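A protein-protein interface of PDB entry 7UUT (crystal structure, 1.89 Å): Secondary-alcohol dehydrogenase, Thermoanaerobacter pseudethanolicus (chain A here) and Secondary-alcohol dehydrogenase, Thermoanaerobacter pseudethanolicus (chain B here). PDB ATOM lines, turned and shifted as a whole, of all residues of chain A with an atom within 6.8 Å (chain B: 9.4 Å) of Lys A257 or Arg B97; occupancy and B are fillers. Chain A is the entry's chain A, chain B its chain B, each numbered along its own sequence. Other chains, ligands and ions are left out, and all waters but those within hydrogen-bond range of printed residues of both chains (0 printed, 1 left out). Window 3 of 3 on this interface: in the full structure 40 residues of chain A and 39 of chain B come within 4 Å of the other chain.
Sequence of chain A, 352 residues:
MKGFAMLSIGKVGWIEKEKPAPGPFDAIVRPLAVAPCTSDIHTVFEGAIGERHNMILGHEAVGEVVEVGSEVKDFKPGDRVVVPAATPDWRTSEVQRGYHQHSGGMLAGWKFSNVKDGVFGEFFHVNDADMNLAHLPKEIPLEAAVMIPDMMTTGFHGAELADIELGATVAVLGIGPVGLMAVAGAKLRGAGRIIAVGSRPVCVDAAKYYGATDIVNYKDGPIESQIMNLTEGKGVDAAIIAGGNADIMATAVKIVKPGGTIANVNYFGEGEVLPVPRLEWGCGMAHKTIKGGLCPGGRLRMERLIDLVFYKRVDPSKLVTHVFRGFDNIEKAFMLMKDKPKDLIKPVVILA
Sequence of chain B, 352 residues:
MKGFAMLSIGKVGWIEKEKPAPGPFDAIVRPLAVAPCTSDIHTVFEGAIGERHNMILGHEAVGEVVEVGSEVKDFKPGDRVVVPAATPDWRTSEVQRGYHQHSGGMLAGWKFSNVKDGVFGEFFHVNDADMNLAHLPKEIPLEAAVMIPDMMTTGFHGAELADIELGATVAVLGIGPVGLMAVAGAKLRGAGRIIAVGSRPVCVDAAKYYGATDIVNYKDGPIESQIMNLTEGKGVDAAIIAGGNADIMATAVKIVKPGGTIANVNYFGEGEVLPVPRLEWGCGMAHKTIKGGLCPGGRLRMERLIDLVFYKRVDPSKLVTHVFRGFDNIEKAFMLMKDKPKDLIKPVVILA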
ATOM      1  N   GLU A 165      17.523  -3.006  18.682  1.00  0.00           N
ATOM      2  CA  GLU A 165      17.136  -3.070  17.281  1.00  0.00           C
ATOM      3  C   GLU A 165      17.292  -4.500  16.771  1.00  0.00           C
ATOM      4  O   GLU A 165      18.050  -5.299  17.325  1.00  0.00           O
ATOM      5  CB  GLU A 165      17.981  -2.104  16.451  1.00  0.00           C
ATOM      6  CG  GLU A 165      17.871  -0.656  16.905  1.00  0.00           C
ATOM      7  CD  GLU A 165      19.092   0.175  16.540  1.00  0.00           C
ATOM      8  OE1 GLU A 165      20.187  -0.407  16.381  1.00  0.00           O
ATOM      9  OE2 GLU A 165      18.958   1.414  16.416  1.00  0.00           O
ATOM     10  N   THR A 169      23.516  -6.858  18.876  1.00  0.00           N
ATOM     11  CA  THR A 169      24.271  -7.684  19.807  1.00  0.00           C
ATOM     12  C   THR A 169      24.043  -7.178  21.221  1.00  0.00           C
ATOM     13  O   THR A 169      24.228  -5.988  21.499  1.00  0.00           O
ATOM     14  CB  THR A 169      25.761  -7.666  19.465  1.00  0.00           C
ATOM     15  OG1 THR A 169      25.962  -8.294  18.192  1.00  0.00           O
ATOM     16  CG2 THR A 169      26.568  -8.392  20.528  1.00  0.00           C
ATOM     17  N   LYS A 234      34.287  -4.109  18.507  1.00  0.00           N
ATOM     18  CA  LYS A 234      33.114  -3.283  18.244  1.00  0.00           C
ATOM     19  C   LYS A 234      32.291  -3.025  19.500  1.00  0.00           C
ATOM     20  O   LYS A 234      31.616  -1.992  19.593  1.00  0.00           O
ATOM     21  CB  LYS A 234      32.230  -3.929  17.171  1.00  0.00           C
ATOM     22  CG  LYS A 234      32.839  -3.936  15.772  1.00  0.00           C
ATOM     23  CD  LYS A 234      31.859  -4.461  14.720  1.00  0.00           C
ATOM     24  CE  LYS A 234      32.000  -5.962  14.489  1.00  0.00           C
ATOM     25  NZ  LYS A 234      31.506  -6.783  15.630  1.00  0.00           N
ATOM     26  N   GLY A 235      32.320  -3.942  20.460  1.00  0.00           N
ATOM     27  CA  GLY A 235      31.434  -3.848  21.597  1.00  0.00           C
ATOM     28  C   GLY A 235      30.045  -4.375  21.279  1.00  0.00           C
ATOM     29  O   GLY A 235      29.788  -4.979  20.232  1.00  0.00           O
ATOM     30  N   VAL A 236      29.132  -4.133  22.214  1.00  0.00           N
ATOM     31  CA  VAL A 236      27.757  -4.586  22.088  1.00  0.00           C
ATOM     32  C   VAL A 236      26.866  -3.370  21.871  1.00  0.00           C
ATOM     33  O   VAL A 236      27.216  -2.236  22.213  1.00  0.00           O
ATOM     34  CB  VAL A 236      27.298  -5.397  23.319  1.00  0.00           C
ATOM     35  CG1 VAL A 236      28.189  -6.615  23.512  1.00  0.00           C
ATOM     36  CG2 VAL A 236      27.304  -4.532  24.568  1.00  0.00           C
ATOM     37  N   ASP A 237      25.700  -3.615  21.269  1.00  0.00           N
ATOM     38  CA  ASP A 237      24.739  -2.543  21.046  1.00  0.00           C
ATOM     39  C   ASP A 237      24.016  -2.156  22.328  1.00  0.00           C
ATOM     40  O   ASP A 237      23.612  -0.998  22.485  1.00  0.00           O
ATOM     41  CB  ASP A 237      23.735  -2.958  19.973  1.00  0.00           C
ATOM     42  CG  ASP A 237      24.396  -3.231  18.634  1.00  0.00           C
ATOM     43  OD1 ASP A 237      24.884  -2.271  17.995  1.00  0.00           O
ATOM     44  OD2 ASP A 237      24.451  -4.416  18.236  1.00  0.00           O
ATOM     45  N   ALA A 238      23.844  -3.101  23.249  1.00  0.00           N
ATOM     46  CA  ALA A 238      23.181  -2.834  24.515  1.00  0.00           C
ATOM     47  C   ALA A 238      23.681  -3.831  25.546  1.00  0.00           C
ATOM     48  O   ALA A 238      23.982  -4.980  25.218  1.00  0.00           O
ATOM     49  CB  ALA A 238      21.656  -2.930  24.395  1.00  0.00           C
ATOM     50  N   ALA A 252      29.670  -2.215  32.189  1.00  0.00           N
ATOM     51  CA  ALA A 252      28.644  -2.026  31.169  1.00  0.00           C
ATOM     52  C   ALA A 252      28.986  -0.858  30.257  1.00  0.00           C
ATOM     53  O   ALA A 252      28.822  -0.945  29.035  1.00  0.00           O
ATOM     54  CB  ALA A 252      27.281  -1.809  31.826  1.00  0.00           C
ATOM     55  N   VAL A 253      29.456   0.247  30.835  1.00  0.00           N
ATOM     56  CA  VAL A 253      29.807   1.414  30.031  1.00  0.00           C
ATOM     57  C   VAL A 253      30.964   1.086  29.095  1.00  0.00           C
ATOM     58  O   VAL A 253      31.005   1.542  27.945  1.00  0.00           O
ATOM     59  CB  VAL A 253      30.134   2.605  30.952  1.00  0.00           C
ATOM     60  CG1 VAL A 253      30.637   3.792  30.145  1.00  0.00           C
ATOM     61  CG2 VAL A 253      28.913   2.988  31.780  1.00  0.00           C
ATOM     62  N   LYS A 254      31.910   0.269  29.564  1.00  0.00           N
ATOM     63  CA  LYS A 254      33.102  -0.027  28.775  1.00  0.00           C
ATOM     64  C   LYS A 254      32.800  -0.929  27.584  1.00  0.00           C
ATOM     65  O   LYS A 254      33.463  -0.815  26.547  1.00  0.00           O
ATOM     66  CB  LYS A 254      34.169  -0.664  29.667  1.00  0.00           C
ATOM     67  CG  LYS A 254      34.729   0.276  30.720  1.00  0.00           C
ATOM     68  CD  LYS A 254      35.648  -0.446  31.691  1.00  0.00           C
ATOM     69  CE  LYS A 254      36.131   0.492  32.790  1.00  0.00           C
ATOM     70  NZ  LYS A 254      36.989  -0.202  33.791  1.00  0.00           N
ATOM     71  N   ILE A 255      31.813  -1.818  27.699  1.00  0.00           N
ATOM     72  CA  ILE A 255      31.549  -2.774  26.627  1.00  0.00           C
ATOM     73  C   ILE A 255      30.496  -2.302  25.629  1.00  0.00           C
ATOM     74  O   ILE A 255      30.420  -2.855  24.523  1.00  0.00           O
ATOM     75  CB  ILE A 255      31.125  -4.141  27.195  1.00  0.00           C
ATOM     76  CG1 ILE A 255      29.770  -4.038  27.899  1.00  0.00           C
ATOM     77  CG2 ILE A 255      32.183  -4.670  28.142  1.00  0.00           C
ATOM     78  CD1 ILE A 255      29.248  -5.366  28.419  1.00  0.00           C
ATOM     79  N   VAL A 256      29.691  -1.302  25.979  1.00  0.00           N
ATOM     80  CA  VAL A 256      28.673  -0.784  25.070  1.00  0.00           C
ATOM     81  C   VAL A 256      29.321   0.184  24.090  1.00  0.00           C
ATOM     82  O   VAL A 256      30.162   1.009  24.469  1.00  0.00           O
ATOM     83  CB  VAL A 256      27.536  -0.117  25.864  1.00  0.00           C
ATOM     84  CG1 VAL A 256      26.591   0.615  24.940  1.00  0.00           C
ATOM     85  CG2 VAL A 256      26.773  -1.157  26.646  1.00  0.00           C
ATOM     86  N   LYS A 257      28.943   0.076  22.818  1.00  0.00           N
ATOM     87  CA  LYS A 257      29.490   0.954  21.799  1.00  0.00           C
ATOM     88  C   LYS A 257      28.873   2.346  21.921  1.00  0.00           C
ATOM     89  O   LYS A 257      27.819   2.514  22.537  1.00  0.00           O
ATOM     90  CB  LYS A 257      29.220   0.383  20.409  1.00  0.00           C
ATOM     91  CG  LYS A 257      27.748   0.321  20.063  1.00  0.00           C
ATOM     92  CD  LYS A 257      27.504  -0.323  18.711  1.00  0.00           C
ATOM     93  CE  LYS A 257      28.044  -1.740  18.657  1.00  0.00           C
ATOM     94  NZ  LYS A 257      27.584  -2.438  17.425  1.00  0.00           N
ATOM     95  N   PRO A 258      29.524   3.366  21.362  1.00  0.00           N
ATOM     96  CA  PRO A 258      28.924   4.708  21.362  1.00  0.00           C
ATOM     97  C   PRO A 258      27.549   4.694  20.714  1.00  0.00           C
ATOM     98  O   PRO A 258      27.347   4.095  19.655  1.00  0.00           O
ATOM     99  CB  PRO A 258      29.926   5.539  20.559  1.00  0.00           C
ATOM    100  CG  PRO A 258      31.225   4.843  20.771  1.00  0.00           C
ATOM    101  CD  PRO A 258      30.905   3.381  20.846  1.00  0.00           C
ATOM    102  N   GLY A 259      26.597   5.358  21.368  1.00  0.00           N
ATOM    103  CA  GLY A 259      25.220   5.351  20.931  1.00  0.00           C
ATOM    104  C   GLY A 259      24.376   4.233  21.507  1.00  0.00           C
ATOM    105  O   GLY A 259      23.151   4.245  21.323  1.00  0.00           O
ATOM    106  N   GLY A 260      24.980   3.277  22.202  1.00  0.00           N
ATOM    107  CA  GLY A 260      24.243   2.175  22.778  1.00  0.00           C
ATOM    108  C   GLY A 260      23.578   2.552  24.085  1.00  0.00           C
ATOM    109  O   GLY A 260      23.585   3.703  24.523  1.00  0.00           O
ATOM    110  N   THR A 261      23.004   1.540  24.729  1.00  0.00           N
ATOM    111  CA  THR A 261      22.211   1.725  25.935  1.00  0.00           C
ATOM    112  C   THR A 261      22.645   0.737  27.006  1.00  0.00           C
ATOM    113  O   THR A 261      22.856  -0.446  26.722  1.00  0.00           O
ATOM    114  CB  THR A 261      20.715   1.540  25.638  1.00  0.00           C
ATOM    115  OG1 THR A 261      20.327   2.434  24.590  1.00  0.00           O
ATOM    116  CG2 THR A 261      19.881   1.834  26.871  1.00  0.00           C
ATOM    117  N   ILE A 262      22.788   1.230  28.234  1.00  0.00           N
ATOM    118  CA  ILE A 262      22.971   0.392  29.414  1.00  0.00           C
ATOM    119  C   ILE A 262      21.643   0.357  30.160  1.00  0.00           C
ATOM    120  O   ILE A 262      21.168   1.389  30.649  1.00  0.00           O
ATOM    121  CB  ILE A 262      24.097   0.916  30.322  1.00  0.00           C
ATOM    122  CG1 ILE A 262      25.461   0.805  29.636  1.00  0.00           C
ATOM    123  CG2 ILE A 262      24.121   0.149  31.627  1.00  0.00           C
ATOM    124  CD1 ILE A 262      25.856   2.041  28.859  1.00  0.00           C
ATOM    125  N   ALA A 286      29.587  10.338  24.853  1.00  0.00           N
ATOM    126  CA  ALA A 286      29.623   9.134  24.032  1.00  0.00           C
ATOM    127  C   ALA A 286      28.244   8.645  23.606  1.00  0.00           C
ATOM    128  O   ALA A 286      28.155   7.607  22.939  1.00  0.00           O
ATOM    129  CB  ALA A 286      30.349   8.008  24.776  1.00  0.00           C
ATOM    130  N   HIS A 287      27.175   9.361  23.966  1.00  0.00           N
ATOM    131  CA  HIS A 287      25.795   8.953  23.671  1.00  0.00           C
ATOM    132  C   HIS A 287      25.474   7.555  24.197  1.00  0.00           C
ATOM    133  O   HIS A 287      24.684   6.824  23.596  1.00  0.00           O
ATOM    134  CB  HIS A 287      25.492   9.032  22.169  1.00  0.00           C
ATOM    135  CG  HIS A 287      25.236  10.423  21.675  1.00  0.00           C
ATOM    136  ND1 HIS A 287      26.228  11.221  21.148  1.00  0.00           N
ATOM    137  CD2 HIS A 287      24.101  11.160  21.640  1.00  0.00           C
ATOM    138  CE1 HIS A 287      25.713  12.385  20.793  1.00  0.00           C
ATOM    139  NE2 HIS A 287      24.425  12.374  21.084  1.00  0.00           N
ATOM    140  N   LYS A 288      26.079   7.169  25.317  1.00  0.00           N
ATOM    141  CA  LYS A 288      25.784   5.892  25.970  1.00  0.00           C
ATOM    142  C   LYS A 288      24.697   6.125  27.016  1.00  0.00           C
ATOM    143  O   LYS A 288      24.975   6.582  28.128  1.00  0.00           O
ATOM    144  CB  LYS A 288      27.049   5.301  26.584  1.00  0.00           C
ATOM    145  CG  LYS A 288      28.118   4.954  25.554  1.00  0.00           C
ATOM    146  CD  LYS A 288      29.304   4.234  26.177  1.00  0.00           C
ATOM    147  CE  LYS A 288      30.439   4.101  25.174  1.00  0.00           C
ATOM    148  NZ  LYS A 288      31.625   3.388  25.737  1.00  0.00           N
ATOM    149  N   TRP B  90      30.619  10.813   6.556  1.00  0.00           N
ATOM    150  CA  TRP B  90      29.238  10.368   6.474  1.00  0.00           C
ATOM    151  C   TRP B  90      29.087   8.981   5.874  1.00  0.00           C
ATOM    152  O   TRP B  90      27.962   8.572   5.570  1.00  0.00           O
ATOM    153  CB  TRP B  90      28.423  11.385   5.680  1.00  0.00           C
ATOM    154  CG  TRP B  90      28.183  12.611   6.478  1.00  0.00           C
ATOM    155  CD1 TRP B  90      28.905  13.767   6.446  1.00  0.00           C
ATOM    156  CD2 TRP B  90      27.153  12.805   7.452  1.00  0.00           C
ATOM    157  NE1 TRP B  90      28.382  14.675   7.337  1.00  0.00           N
ATOM    158  CE2 TRP B  90      27.306  14.108   7.967  1.00  0.00           C
ATOM    159  CE3 TRP B  90      26.114  12.004   7.934  1.00  0.00           C
ATOM    160  CZ2 TRP B  90      26.460  14.626   8.941  1.00  0.00           C
ATOM    161  CZ3 TRP B  90      25.276  12.521   8.900  1.00  0.00           C
ATOM    162  CH2 TRP B  90      25.453  13.821   9.393  1.00  0.00           C
ATOM    163  N   THR B  92      30.096   5.647   7.172  1.00  0.00           N
ATOM    164  CA  THR B  92      30.530   4.676   8.169  1.00  0.00           C
ATOM    165  C   THR B  92      29.317   3.905   8.670  1.00  0.00           C
ATOM    166  O   THR B  92      28.170   4.241   8.366  1.00  0.00           O
ATOM    167  CB  THR B  92      31.231   5.346   9.359  1.00  0.00           C
ATOM    168  OG1 THR B  92      30.324   6.261   9.990  1.00  0.00           O
ATOM    169  CG2 THR B  92      32.486   6.094   8.911  1.00  0.00           C
ATOM    170  N   SER B  93      29.582   2.865   9.464  1.00  0.00           N
ATOM    171  CA  SER B  93      28.487   2.093  10.040  1.00  0.00           C
ATOM    172  C   SER B  93      27.769   2.875  11.132  1.00  0.00           C
ATOM    173  O   SER B  93      26.547   2.753  11.278  1.00  0.00           O
ATOM    174  CB  SER B  93      29.001   0.761  10.590  1.00  0.00           C
ATOM    175  OG  SER B  93      29.942   0.961  11.630  1.00  0.00           O
ATOM    176  N   GLU B  94      28.502   3.684  11.903  1.00  0.00           N
ATOM    177  CA  GLU B  94      27.874   4.473  12.959  1.00  0.00           C
ATOM    178  C   GLU B  94      26.903   5.507  12.404  1.00  0.00           C
ATOM    179  O   GLU B  94      25.990   5.931  13.124  1.00  0.00           O
ATOM    180  CB  GLU B  94      28.935   5.171  13.814  1.00  0.00           C
ATOM    181  CG  GLU B  94      29.829   4.226  14.609  1.00  0.00           C
ATOM    182  CD  GLU B  94      31.096   3.843  13.864  1.00  0.00           C
ATOM    183  OE1 GLU B  94      31.246   4.243  12.689  1.00  0.00           O
ATOM    184  OE2 GLU B  94      31.946   3.146  14.461  1.00  0.00           O
ATOM    185  N   VAL B  95      27.083   5.928  11.150  1.00  0.00           N
ATOM    186  CA  VAL B  95      26.131   6.847  10.534  1.00  0.00           C
ATOM    187  C   VAL B  95      24.830   6.122  10.213  1.00  0.00           C
ATOM    188  O   VAL B  95      23.737   6.680  10.376  1.00  0.00           O
ATOM    189  CB  VAL B  95      26.756   7.502   9.289  1.00  0.00           C
ATOM    190  CG1 VAL B  95      25.706   8.256   8.488  1.00  0.00           C
ATOM    191  CG2 VAL B  95      27.885   8.438   9.703  1.00  0.00           C
ATOM    192  N   GLN B  96      24.919   4.863   9.768  1.00  0.00           N
ATOM    193  CA  GLN B  96      23.718   4.065   9.538  1.00  0.00           C
ATOM    194  C   GLN B  96      22.994   3.736  10.842  1.00  0.00           C
ATOM    195  O   GLN B  96      21.805   3.399  10.805  1.00  0.00           O
ATOM    196  CB  GLN B  96      24.063   2.776   8.781  1.00  0.00           C
ATOM    197  CG  GLN B  96      24.766   2.998   7.438  1.00  0.00           C
ATOM    198  CD  GLN B  96      24.796   1.755   6.546  1.00  0.00           C
ATOM    199  OE1 GLN B  96      23.962   0.859   6.667  1.00  0.00           O
ATOM    200  NE2 GLN B  96      25.763   1.705   5.642  1.00  0.00           N
ATOM    201  N   ARG B  97      23.683   3.812  11.986  1.00  0.00           N
ATOM    202  CA  ARG B  97      23.046   3.667  13.293  1.00  0.00           C
ATOM    203  C   ARG B  97      22.436   4.965  13.805  1.00  0.00           C
ATOM    204  O   ARG B  97      21.731   4.939  14.821  1.00  0.00           O
ATOM    205  CB  ARG B  97      24.043   3.142  14.335  1.00  0.00           C
ATOM    206  CG  ARG B  97      24.337   1.652  14.235  1.00  0.00           C
ATOM    207  CD  ARG B  97      24.983   1.101  15.504  1.00  0.00           C
ATOM    208  NE  ARG B  97      26.273   1.718  15.792  1.00  0.00           N
ATOM    209  CZ  ARG B  97      26.511   2.508  16.830  1.00  0.00           C
ATOM    210  NH1 ARG B  97      25.566   2.798  17.710  1.00  0.00           N
ATOM    211  NH2 ARG B  97      27.729   3.021  16.990  1.00  0.00           N
ATOM    212  N   GLY B  98      22.706   6.094  13.157  1.00  0.00           N
ATOM    213  CA  GLY B  98      22.136   7.358  13.574  1.00  0.00           C
ATOM    214  C   GLY B  98      22.973   8.165  14.538  1.00  0.00           C
ATOM    215  O   GLY B  98      22.425   9.027  15.236  1.00  0.00           O
ATOM    216  N   TYR B  99      24.286   7.916  14.608  1.00  0.00           N
ATOM    217  CA  TYR B  99      25.188   8.635  15.512  1.00  0.00           C
ATOM    218  C   TYR B  99      26.404   9.095  14.714  1.00  0.00           C
ATOM    219  O   TYR B  99      27.489   8.518  14.815  1.00  0.00           O
ATOM    220  CB  TYR B  99      25.575   7.763  16.707  1.00  0.00           C
ATOM    221  CG  TYR B  99      24.432   7.554  17.667  1.00  0.00           C
ATOM    222  CD1 TYR B  99      24.140   8.501  18.640  1.00  0.00           C
ATOM    223  CD2 TYR B  99      23.626   6.426  17.582  1.00  0.00           C
ATOM    224  CE1 TYR B  99      23.087   8.323  19.517  1.00  0.00           C
ATOM    225  CE2 TYR B  99      22.569   6.240  18.453  1.00  0.00           C
ATOM    226  CZ  TYR B  99      22.303   7.191  19.418  1.00  0.00           C
ATOM    227  OH  TYR B  99      21.252   7.013  20.290  1.00  0.00           O
ATOM    228  N   HIS B 100      26.208  10.146  13.912  1.00  0.00           N
ATOM    229  CA  HIS B 100      27.301  10.691  13.115  1.00  0.00           C
ATOM    230  C   HIS B 100      28.389  11.301  13.991  1.00  0.00           C
ATOM    231  O   HIS B 100      29.557  11.342  13.586  1.00  0.00           O
ATOM    232  CB  HIS B 100      26.757  11.733  12.139  1.00  0.00           C
ATOM    233  CG  HIS B 100      26.156  12.931  12.810  1.00  0.00           C
ATOM    234  ND1 HIS B 100      24.798  13.080  12.990  1.00  0.00           N
ATOM    235  CD2 HIS B 100      26.730  14.037  13.345  1.00  0.00           C
ATOM    236  CE1 HIS B 100      24.560  14.225  13.608  1.00  0.00           C
ATOM    237  NE2 HIS B 100      25.716  14.824  13.835  1.00  0.00           N
ATOM    238  N   GLN B 101      28.035  11.759  15.198  1.00  0.00           N
ATOM    239  CA  GLN B 101      29.035  12.306  16.109  1.00  0.00           C
ATOM    240  C   GLN B 101      30.136  11.301  16.415  1.00  0.00           C
ATOM    241  O   GLN B 101      31.247  11.704  16.780  1.00  0.00           O
ATOM    242  CB  GLN B 101      28.381  12.758  17.418  1.00  0.00           C
ATOM    243  CG  GLN B 101      27.312  13.826  17.259  1.00  0.00           C
ATOM    244  CD  GLN B 101      25.911  13.248  17.236  1.00  0.00           C
ATOM    245  OE1 GLN B 101      25.651  12.246  16.571  1.00  0.00           O
ATOM    246  NE2 GLN B 101      24.998  13.881  17.966  1.00  0.00           N
ATOM    247  N   HIS B 102      29.852  10.007  16.266  1.00  0.00           N
ATOM    248  CA  HIS B 102      30.812   8.946  16.536  1.00  0.00           C
ATOM    249  C   HIS B 102      31.153   8.174  15.266  1.00  0.00           C
ATOM    250  O   HIS B 102      31.485   6.988  15.316  1.00  0.00           O
ATOM    251  CB  HIS B 102      30.278   8.014  17.621  1.00  0.00           C
ATOM    252  CG  HIS B 102      29.731   8.744  18.804  1.00  0.00           C
ATOM    253  ND1 HIS B 102      30.536   9.419  19.697  1.00  0.00           N
ATOM    254  CD2 HIS B 102      28.458   8.935  19.225  1.00  0.00           C
ATOM    255  CE1 HIS B 102      29.783   9.983  20.625  1.00  0.00           C
ATOM    256  NE2 HIS B 102      28.520   9.703  20.362  1.00  0.00           N
ATOM    257  N   SER B 103      31.073   8.846  14.119  1.00  0.00           N
ATOM    258  CA  SER B 103      31.379   8.233  12.831  1.00  0.00           C
ATOM    259  C   SER B 103      32.869   7.909  12.760  1.00  0.00           C
ATOM    260  O   SER B 103      33.703   8.806  12.601  1.00  0.00           O
ATOM    261  CB  SER B 103      30.964   9.176  11.706  1.00  0.00           C
ATOM    262  OG  SER B 103      31.270   8.636  10.436  1.00  0.00           O
ATOM    263  N   GLY B 104      33.205   6.624  12.860  1.00  0.00           N
ATOM    264  CA  GLY B 104      34.586   6.187  12.847  1.00  0.00           C
ATOM    265  C   GLY B 104      35.229   6.028  14.208  1.00  0.00           C
ATOM    266  O   GLY B 104      36.453   5.860  14.279  1.00  0.00           O
ATOM    267  N   GLY B 105      34.451   6.076  15.287  1.00  0.00           N
ATOM    268  CA  GLY B 105      34.993   5.956  16.627  1.00  0.00           C
ATOM    269  C   GLY B 105      34.340   6.931  17.586  1.00  0.00           C
ATOM    270  O   GLY B 105      33.636   7.845  17.151  1.00  0.00           O
ATOM    271  N   MET B 106      34.563   6.755  18.886  1.00  0.00           N
ATOM    272  CA  MET B 106      33.957   7.641  19.873  1.00  0.00           C
ATOM    273  C   MET B 106      34.442   9.074  19.676  1.00  0.00           C
ATOM    274  O   MET B 106      35.647   9.335  19.625  1.00  0.00           O
ATOM    275  CB  MET B 106      34.282   7.154  21.284  1.00  0.00           C
ATOM    276  CG  MET B 106      33.438   7.792  22.376  1.00  0.00           C
ATOM    277  SD  MET B 106      33.683   6.974  23.965  1.00  0.00           S
ATOM    278  CE  MET B 106      35.446   7.205  24.205  1.00  0.00           C
ATOM    279  N   LEU B 107      33.486   9.999  19.538  1.00  0.00           N
ATOM    280  CA  LEU B 107      33.740  11.427  19.333  1.00  0.00           C
ATOM    281  C   LEU B 107      34.472  11.708  18.025  1.00  0.00           C
ATOM    282  O   LEU B 107      35.003  12.806  17.837  1.00  0.00           O
ATOM    283  CB  LEU B 107      34.515  12.040  20.509  1.00  0.00           C
ATOM    284  CG  LEU B 107      33.982  11.796  21.925  1.00  0.00           C
ATOM    285  CD1 LEU B 107      34.888  12.447  22.964  1.00  0.00           C
ATOM    286  CD2 LEU B 107      32.559  12.307  22.062  1.00  0.00           C
ATOM    287  N   GLY B 292      24.238  11.398  27.732  1.00  0.00           N
ATOM    288  CA  GLY B 292      25.351  12.307  27.534  1.00  0.00           C
ATOM    289  C   GLY B 292      25.915  12.216  26.133  1.00  0.00           C
ATOM    290  O   GLY B 292      26.443  11.168  25.755  1.00  0.00           O
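Of chain B, only Arg B97 comes within 4 Å of Lys A257. Arg B97 touches just these residues of chain A: Lys A257 and Pro A258. No residue of chain B comes within 4 Å of Gly A235. Asp A237 touches none of the printed residues of chain B. No residue of chain B comes within 4 Å of Val A256. Of chain B, only Arg B97, His B102 and Met B106 come within 4 Å of Pro A258. Gly A259 touches just one residue of chain B: Tyr B99. No residue of chain B comes within 4 Å of Gly A260. Printed residues of chain B within 4 Å of His A287: Tyr B99 (3.6 Å), Gln B101 (3.3 Å), His B102 (2.9 Å) and Gly B292 (2.6 Å). Printed residues of chain A within 4 Å of Gln B101: His A287 (3.3 Å). The nearest residue of chain B that does not touch Lys A257 is Glu B94 (6.6 Å). The nearest printed residue of chain A that does not touch Gln B101 is Pro A258 (7.1 Å).
Of the 21 printed residues of chain A, 5 touch a printed residue of chain B. Printed residues of chain A that touch a printed residue of chain B: Lys A257, Pro A258, Gly A259, Ala A286 and His A287. Hydrophobic or aromatic side chains of chain A that line the printed part of chain B: Pro A258, Ala A286 and His A287. Along chain A the printed residues that touch a printed residue of chain B span positions 257 to 287. Of the 18 printed residues of chain B, 6 touch a printed residue of chain A. Hydrophobic or aromatic side chains of chain B within 4 Å of the printed part of chain A: Tyr B99, His B102 and Met B106.
The backbone carbonyl oxygen (O) of Ala A286 is in hydrogen-bond range of a ring nitrogen (NE2) of His B102. N of His A287 sits at hydrogen-bond distance from O of Gly B292 (2.6 Å). N of Ala A286 lies within hydrogen-bond range of O of Gly B292, 3.4 Å away. The backbone carbonyl oxygen (O) of Pro A258 is in hydrogen-bond range of the guanidinium group (NH2) of Arg B97 (2.9 Å). A ring nitrogen (ND1) of His A287 is in hydrogen-bond range of a ring nitrogen (NE2) of His B102 (2.9 Å).
Lys A257 touches Arg B97 (CD to CZ, 3.5 Å). His B102 touches Pro A258. CG of Pro A258 touches CB of Met B106 (3.9 Å). Tyr B99 touches Gly A259 (OH to O, 3.5 Å). Met B106 touches Ala A286. CB of His A287 touches CE1 of Tyr B99 (3.6 Å). CE1 of His A287 touches NE2 of Gln B101 (3.3 Å).
The side-chain amino group (NZ) of Lys A257 lies within salt-bridge range of the side-chain carboxylate (OD1) of Asp A237, at 2.8 Å. N of Leu B107 sits at hydrogen-bond distance from ND1 of His B102, 3.0 Å away. The backbone carbonyl oxygen of Val A236 sits at hydrogen-bond distance from the backbone NH of Lys A257 (2.9 Å). The backbone carbonyl oxygen (O) of Glu B94 is in hydrogen-bond range of the backbone NH (N) of Tyr B99 (3.0 Å). The backbone NH (N) of Gly A259 lies close to the backbone carbonyl oxygen (O) of His A287. The backbone NH of Gly A259 is in hydrogen-bond range of the backbone carbonyl oxygen of Ala A286, at 3.2 Å.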
